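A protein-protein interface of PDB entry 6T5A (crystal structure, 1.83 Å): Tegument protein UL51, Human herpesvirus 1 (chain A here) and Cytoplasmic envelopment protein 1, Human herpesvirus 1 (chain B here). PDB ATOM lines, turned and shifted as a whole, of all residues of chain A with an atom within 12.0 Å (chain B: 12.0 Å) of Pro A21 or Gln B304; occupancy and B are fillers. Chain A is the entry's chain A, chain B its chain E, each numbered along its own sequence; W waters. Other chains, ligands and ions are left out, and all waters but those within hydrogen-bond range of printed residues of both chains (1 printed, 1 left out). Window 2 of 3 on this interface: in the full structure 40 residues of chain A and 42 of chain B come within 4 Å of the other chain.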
ATOM      1  N   ALA A  18      -8.581  -7.794 -24.091  1.00  0.00           N
ATOM      2  CA  ALA A  18      -7.930  -9.023 -23.640  1.00  0.00           C
ATOM      3  C   ALA A  18      -8.701 -10.290 -24.050  1.00  0.00           C
ATOM      4  O   ALA A  18      -8.082 -11.341 -24.246  1.00  0.00           O
ATOM      5  CB  ALA A  18      -7.751  -8.993 -22.128  1.00  0.00           C
ATOM      6  N   ALA A  19     -10.045 -10.183 -24.154  1.00  0.00           N
ATOM      7  CA  ALA A  19     -10.968 -11.273 -24.469  1.00  0.00           C
ATOM      8  C   ALA A  19     -10.732 -11.941 -25.816  1.00  0.00           C
ATOM      9  O   ALA A  19     -10.584 -11.267 -26.841  1.00  0.00           O
ATOM     10  CB  ALA A  19     -12.410 -10.792 -24.363  1.00  0.00           C
ATOM     11  N   VAL A  20     -10.698 -13.278 -25.806  1.00  0.00           N
ATOM     12  CA  VAL A  20     -10.530 -14.080 -27.019  1.00  0.00           C
ATOM     13  C   VAL A  20     -11.941 -14.439 -27.528  1.00  0.00           C
ATOM     14  O   VAL A  20     -12.698 -15.090 -26.812  1.00  0.00           O
ATOM     15  CB  VAL A  20      -9.636 -15.329 -26.791  1.00  0.00           C
ATOM     16  CG1 VAL A  20      -9.434 -16.105 -28.093  1.00  0.00           C
ATOM     17  CG2 VAL A  20      -8.288 -14.931 -26.180  1.00  0.00           C
ATOM     18  N   PRO A  21     -12.336 -13.975 -28.724  1.00  0.00           N
ATOM     19  CA  PRO A  21     -13.698 -14.284 -29.205  1.00  0.00           C
ATOM     20  C   PRO A  21     -13.849 -15.753 -29.614  1.00  0.00           C
ATOM     21  O   PRO A  21     -12.854 -16.371 -30.004  1.00  0.00           O
ATOM     22  CB  PRO A  21     -13.869 -13.357 -30.420  1.00  0.00           C
ATOM     23  CG  PRO A  21     -12.492 -13.110 -30.909  1.00  0.00           C
ATOM     24  CD  PRO A  21     -11.578 -13.161 -29.702  1.00  0.00           C
ATOM     25  N   PRO A  22     -15.081 -16.305 -29.620  1.00  0.00           N
ATOM     26  CA  PRO A  22     -15.274 -17.701 -30.066  1.00  0.00           C
ATOM     27  C   PRO A  22     -14.685 -17.979 -31.447  1.00  0.00           C
ATOM     28  O   PRO A  22     -14.133 -19.047 -31.648  1.00  0.00           O
ATOM     29  CB  PRO A  22     -16.787 -17.833 -30.106  1.00  0.00           C
ATOM     30  CG  PRO A  22     -17.243 -16.952 -28.988  1.00  0.00           C
ATOM     31  CD  PRO A  22     -16.361 -15.734 -29.154  1.00  0.00           C
ATOM     32  N   SER A  23     -14.739 -16.999 -32.385  1.00  0.00           N
ATOM     33  CA  SER A  23     -14.199 -17.176 -33.736  1.00  0.00           C
ATOM     34  C   SER A  23     -12.709 -17.538 -33.745  1.00  0.00           C
ATOM     35  O   SER A  23     -12.263 -18.208 -34.664  1.00  0.00           O
ATOM     36  CB  SER A  23     -14.477 -15.952 -34.600  1.00  0.00           C
ATOM     37  OG  SER A  23     -13.921 -14.782 -34.034  1.00  0.00           O
ATOM     38  N   GLU A  24     -11.963 -17.152 -32.698  1.00  0.00           N
ATOM     39  CA  GLU A  24     -10.549 -17.504 -32.539  1.00  0.00           C
ATOM     40  C   GLU A  24     -10.331 -18.712 -31.613  1.00  0.00           C
ATOM     41  O   GLU A  24      -9.385 -19.456 -31.804  1.00  0.00           O
ATOM     42  CB  GLU A  24      -9.712 -16.301 -32.047  1.00  0.00           C
ATOM     43  CG  GLU A  24      -9.513 -15.205 -33.081  1.00  0.00           C
ATOM     44  CD  GLU A  24      -8.975 -15.641 -34.429  1.00  0.00           C
ATOM     45  OE1 GLU A  24      -7.987 -16.408 -34.472  1.00  0.00           O
ATOM     46  OE2 GLU A  24      -9.557 -15.216 -35.449  1.00  0.00           O
ATOM     47  N   ALA A  25     -11.182 -18.907 -30.608  1.00  0.00           N
ATOM     48  CA  ALA A  25     -11.055 -20.036 -29.693  1.00  0.00           C
ATOM     49  C   ALA A  25     -12.458 -20.477 -29.347  1.00  0.00           C
ATOM     50  O   ALA A  25     -13.095 -19.943 -28.426  1.00  0.00           O
ATOM     51  CB  ALA A  25     -10.247 -19.641 -28.443  1.00  0.00           C
ATOM     52  N   GLU A  26     -12.977 -21.401 -30.168  1.00  0.00           N
ATOM     53  CA  GLU A  26     -14.352 -21.881 -30.047  1.00  0.00           C
ATOM     54  C   GLU A  26     -14.623 -22.496 -28.704  1.00  0.00           C
ATOM     55  O   GLU A  26     -13.849 -23.339 -28.249  1.00  0.00           O
ATOM     56  CB  GLU A  26     -14.757 -22.830 -31.192  1.00  0.00           C
ATOM     57  CG  GLU A  26     -14.849 -22.145 -32.555  1.00  0.00           C
ATOM     58  CD  GLU A  26     -15.928 -21.104 -32.825  1.00  0.00           C
ATOM     59  OE1 GLU A  26     -16.808 -20.866 -31.968  1.00  0.00           O
ATOM     60  OE2 GLU A  26     -15.863 -20.492 -33.909  1.00  0.00           O
ATOM     61  N   PRO A  27     -15.706 -22.066 -28.039  1.00  0.00           N
ATOM     62  CA  PRO A  27     -16.033 -22.672 -26.741  1.00  0.00           C
ATOM     63  C   PRO A  27     -16.504 -24.115 -26.890  1.00  0.00           C
ATOM     64  O   PRO A  27     -16.968 -24.532 -27.959  1.00  0.00           O
ATOM     65  CB  PRO A  27     -17.124 -21.756 -26.165  1.00  0.00           C
ATOM     66  CG  PRO A  27     -17.656 -20.979 -27.311  1.00  0.00           C
ATOM     67  CD  PRO A  27     -16.709 -21.063 -28.454  1.00  0.00           C
ATOM     68  N   ARG A  28     -16.354 -24.883 -25.808  1.00  0.00           N
ATOM     69  CA  ARG A  28     -16.757 -26.287 -25.716  1.00  0.00           C
ATOM     70  C   ARG A  28     -17.784 -26.365 -24.583  1.00  0.00           C
ATOM     71  O   ARG A  28     -17.662 -25.659 -23.568  1.00  0.00           O
ATOM     72  CB  ARG A  28     -15.545 -27.168 -25.354  1.00  0.00           C
ATOM     73  CG  ARG A  28     -14.480 -27.304 -26.452  1.00  0.00           C
ATOM     74  CD  ARG A  28     -13.318 -28.170 -26.008  1.00  0.00           C
ATOM     75  NE  ARG A  28     -12.104 -27.926 -26.795  1.00  0.00           N
ATOM     76  CZ  ARG A  28     -11.620 -28.757 -27.716  1.00  0.00           C
ATOM     77  NH1 ARG A  28     -12.234 -29.908 -27.972  1.00  0.00           N
ATOM     78  NH2 ARG A  28     -10.519 -28.444 -28.388  1.00  0.00           N
ATOM     79  N   LEU A  29     -18.799 -27.196 -24.777  1.00  0.00           N
ATOM     80  CA  LEU A  29     -19.811 -27.469 -23.779  1.00  0.00           C
ATOM     81  C   LEU A  29     -19.783 -28.963 -23.469  1.00  0.00           C
ATOM     82  O   LEU A  29     -19.990 -29.770 -24.374  1.00  0.00           O
ATOM     83  CB  LEU A  29     -21.200 -27.023 -24.254  1.00  0.00           C
ATOM     84  CG  LEU A  29     -22.402 -27.448 -23.379  1.00  0.00           C
ATOM     85  CD1 LEU A  29     -22.313 -26.857 -21.958  1.00  0.00           C
ATOM     86  CD2 LEU A  29     -23.706 -27.039 -24.038  1.00  0.00           C
ATOM     87  N   GLN A  30     -19.529 -29.320 -22.198  1.00  0.00           N
ATOM     88  CA  GLN A  30     -19.520 -30.713 -21.739  1.00  0.00           C
ATOM     89  C   GLN A  30     -20.671 -30.883 -20.777  1.00  0.00           C
ATOM     90  O   GLN A  30     -20.896 -30.002 -19.940  1.00  0.00           O
ATOM     91  CB  GLN A  30     -18.192 -31.054 -21.047  1.00  0.00           C
ATOM     92  CG  GLN A  30     -16.984 -31.072 -21.984  1.00  0.00           C
ATOM     93  CD  GLN A  30     -15.690 -31.337 -21.251  1.00  0.00           C
ATOM     94  OE1 GLN A  30     -15.574 -31.161 -20.036  1.00  0.00           O
ATOM     95  NE2 GLN A  30     -14.673 -31.753 -21.984  1.00  0.00           N
ATOM     96  N   GLU B 300     -23.222 -28.920 -16.361  1.00  0.00           N
ATOM     97  CA  GLU B 300     -22.812 -28.377 -17.651  1.00  0.00           C
ATOM     98  C   GLU B 300     -21.570 -27.532 -17.442  1.00  0.00           C
ATOM     99  O   GLU B 300     -21.553 -26.682 -16.556  1.00  0.00           O
ATOM    100  CB  GLU B 300     -23.929 -27.538 -18.290  1.00  0.00           C
ATOM    101  CG  GLU B 300     -25.142 -28.375 -18.645  1.00  0.00           C
ATOM    102  CD  GLU B 300     -26.349 -27.543 -18.998  1.00  0.00           C
ATOM    103  OE1 GLU B 300     -27.024 -27.047 -18.069  1.00  0.00           O
ATOM    104  OE2 GLU B 300     -26.610 -27.370 -20.209  1.00  0.00           O
ATOM    105  N   VAL B 301     -20.528 -27.768 -18.263  1.00  0.00           N
ATOM    106  CA  VAL B 301     -19.241 -27.067 -18.160  1.00  0.00           C
ATOM    107  C   VAL B 301     -18.964 -26.387 -19.489  1.00  0.00           C
ATOM    108  O   VAL B 301     -18.900 -27.064 -20.509  1.00  0.00           O
ATOM    109  CB  VAL B 301     -18.096 -28.062 -17.759  1.00  0.00           C
ATOM    110  CG1 VAL B 301     -16.766 -27.344 -17.562  1.00  0.00           C
ATOM    111  CG2 VAL B 301     -18.467 -28.857 -16.497  1.00  0.00           C
ATOM    112  N   LEU B 302     -18.797 -25.062 -19.480  1.00  0.00           N
ATOM    113  CA  LEU B 302     -18.527 -24.261 -20.682  1.00  0.00           C
ATOM    114  C   LEU B 302     -17.159 -23.627 -20.569  1.00  0.00           C
ATOM    115  O   LEU B 302     -16.909 -22.928 -19.592  1.00  0.00           O
ATOM    116  CB  LEU B 302     -19.549 -23.113 -20.797  1.00  0.00           C
ATOM    117  CG  LEU B 302     -20.822 -23.294 -21.585  1.00  0.00           C
ATOM    118  CD1 LEU B 302     -21.697 -22.043 -21.432  1.00  0.00           C
ATOM    119  CD2 LEU B 302     -20.532 -23.522 -23.070  1.00  0.00           C
ATOM    120  N   PHE B 303     -16.291 -23.797 -21.576  1.00  0.00           N
ATOM    121  CA  PHE B 303     -14.946 -23.200 -21.535  1.00  0.00           C
ATOM    122  C   PHE B 303     -14.395 -22.955 -22.920  1.00  0.00           C
ATOM    123  O   PHE B 303     -14.831 -23.598 -23.875  1.00  0.00           O
ATOM    124  CB  PHE B 303     -13.958 -24.085 -20.725  1.00  0.00           C
ATOM    125  CG  PHE B 303     -13.819 -25.501 -21.221  1.00  0.00           C
ATOM    126  CD1 PHE B 303     -14.724 -26.486 -20.831  1.00  0.00           C
ATOM    127  CD2 PHE B 303     -12.763 -25.864 -22.049  1.00  0.00           C
ATOM    128  CE1 PHE B 303     -14.598 -27.796 -21.297  1.00  0.00           C
ATOM    129  CE2 PHE B 303     -12.628 -27.183 -22.493  1.00  0.00           C
ATOM    130  CZ  PHE B 303     -13.544 -28.137 -22.116  1.00  0.00           C
ATOM    131  N   GLN B 304     -13.414 -22.052 -23.024  1.00  0.00           N
ATOM    132  CA  GLN B 304     -12.699 -21.728 -24.259  1.00  0.00           C
ATOM    133  C   GLN B 304     -11.245 -22.182 -24.132  1.00  0.00           C
ATOM    134  O   GLN B 304     -10.829 -22.523 -23.005  1.00  0.00           O
ATOM    135  CB  GLN B 304     -12.752 -20.228 -24.536  1.00  0.00           C
ATOM    136  CG  GLN B 304     -14.046 -19.779 -25.152  1.00  0.00           C
ATOM    137  CD  GLN B 304     -14.033 -18.301 -25.378  1.00  0.00           C
ATOM    138  OE1 GLN B 304     -14.451 -17.528 -24.519  1.00  0.00           O
ATOM    139  NE2 GLN B 304     -13.534 -17.879 -26.522  1.00  0.00           N
ATOM    140  OXT GLN B 304     -10.515 -22.192 -25.152  1.00  0.00           O
HETATM  141  O   HOH W   1     -11.179 -23.213 -27.569  1.00  0.00           O
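NE2 of Gln B304 sits at hydrogen-bond distance from O of Val A20 (2.9 Å). The side-chain amide nitrogen (NE2) of Gln B304 is in hydrogen-bond range of the backbone carbonyl oxygen (O) of Ala A25, 2.8 Å away. N of Arg A28 lies within hydrogen-bond range of O of Phe B303 (2.8 Å). The backbone NH of Val B301 sits at hydrogen-bond distance from the backbone carbonyl oxygen of Gln A30 (2.8 Å).
Among the printed residues, pairs that only touch across the chains: Pro A27 with Phe B303 (3.2 Å), Arg A28 with Leu B302 (3.3 Å), Gln A30 with Glu B300 (3.4 Å), Leu A29 with Val B301 (3.4 Å), Arg A28 with Val B301 (3.6 Å), Gln A30 with Phe B303 (3.7 Å), Leu A29 with Leu B302 (3.8 Å), Pro A21 with Gln B304 (3.8 Å), Pro A27 with Gln B304 (3.8 Å) and Pro A22 with Gln B304 (3.8 Å).
Pro A21 touches just one residue of chain B: Gln B304 (3.8 Å). Printed residues of chain A within 4 Å of Gln B304: Val A20, Pro A21, Pro A22, Ala A25 and Pro A27. No residue of chain B comes within 4 Å of Ala A19. Of chain B, only Gln B304 (2.9 Å) comes within 4 Å of Val A20. Pro A22 touches just one residue of chain B: Gln B304 (3.8 Å). No residue of chain B comes within 4 Å of Ser A23. No residue of chain B comes within 4 Å of Glu A24. No residue of chain B comes within 4 Å of Glu A26. Pro A27 touches two residues of chain B. Printed residues of chain B within 4 Å of Gln A30: Glu B300 (3.4 Å), Val B301 (2.8 Å) and Phe B303 (3.7 Å). Of the printed residues of chain A, Leu B302 touches Arg A28 (3.3 Å) and Leu A29 (3.8 Å). Printed residues of chain A within 4 Å of Glu B300: Gln A30. Printed residues of chain B within 4 Å of Leu A29: Val B301 and Leu B302. The nearest residue of chain B that does not touch Pro A21 is Phe B303 (9.7 Å). The nearest residue of chain A that does not touch Gln B304 is Glu A26 (4.5 Å). The nearest printed residue of chain B that does not touch Arg A28 is Gln B304 (4.9 Å).
Hydrophobic or aromatic side chains of chain A that line the printed part of chain B: Pro A27 and Leu A29. Of the 5 printed residues of chain B, 5 touch a printed residue of chain A. Hydrophobic or aromatic side chains of chain B within 4 Å of the printed part of chain A: Leu B302 and Phe B303.
Water W1 bridges the chain-end carboxylate of Gln B304 (2.7 Å) and the backbone carbonyl oxygen of Glu A26 (2.8 Å).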
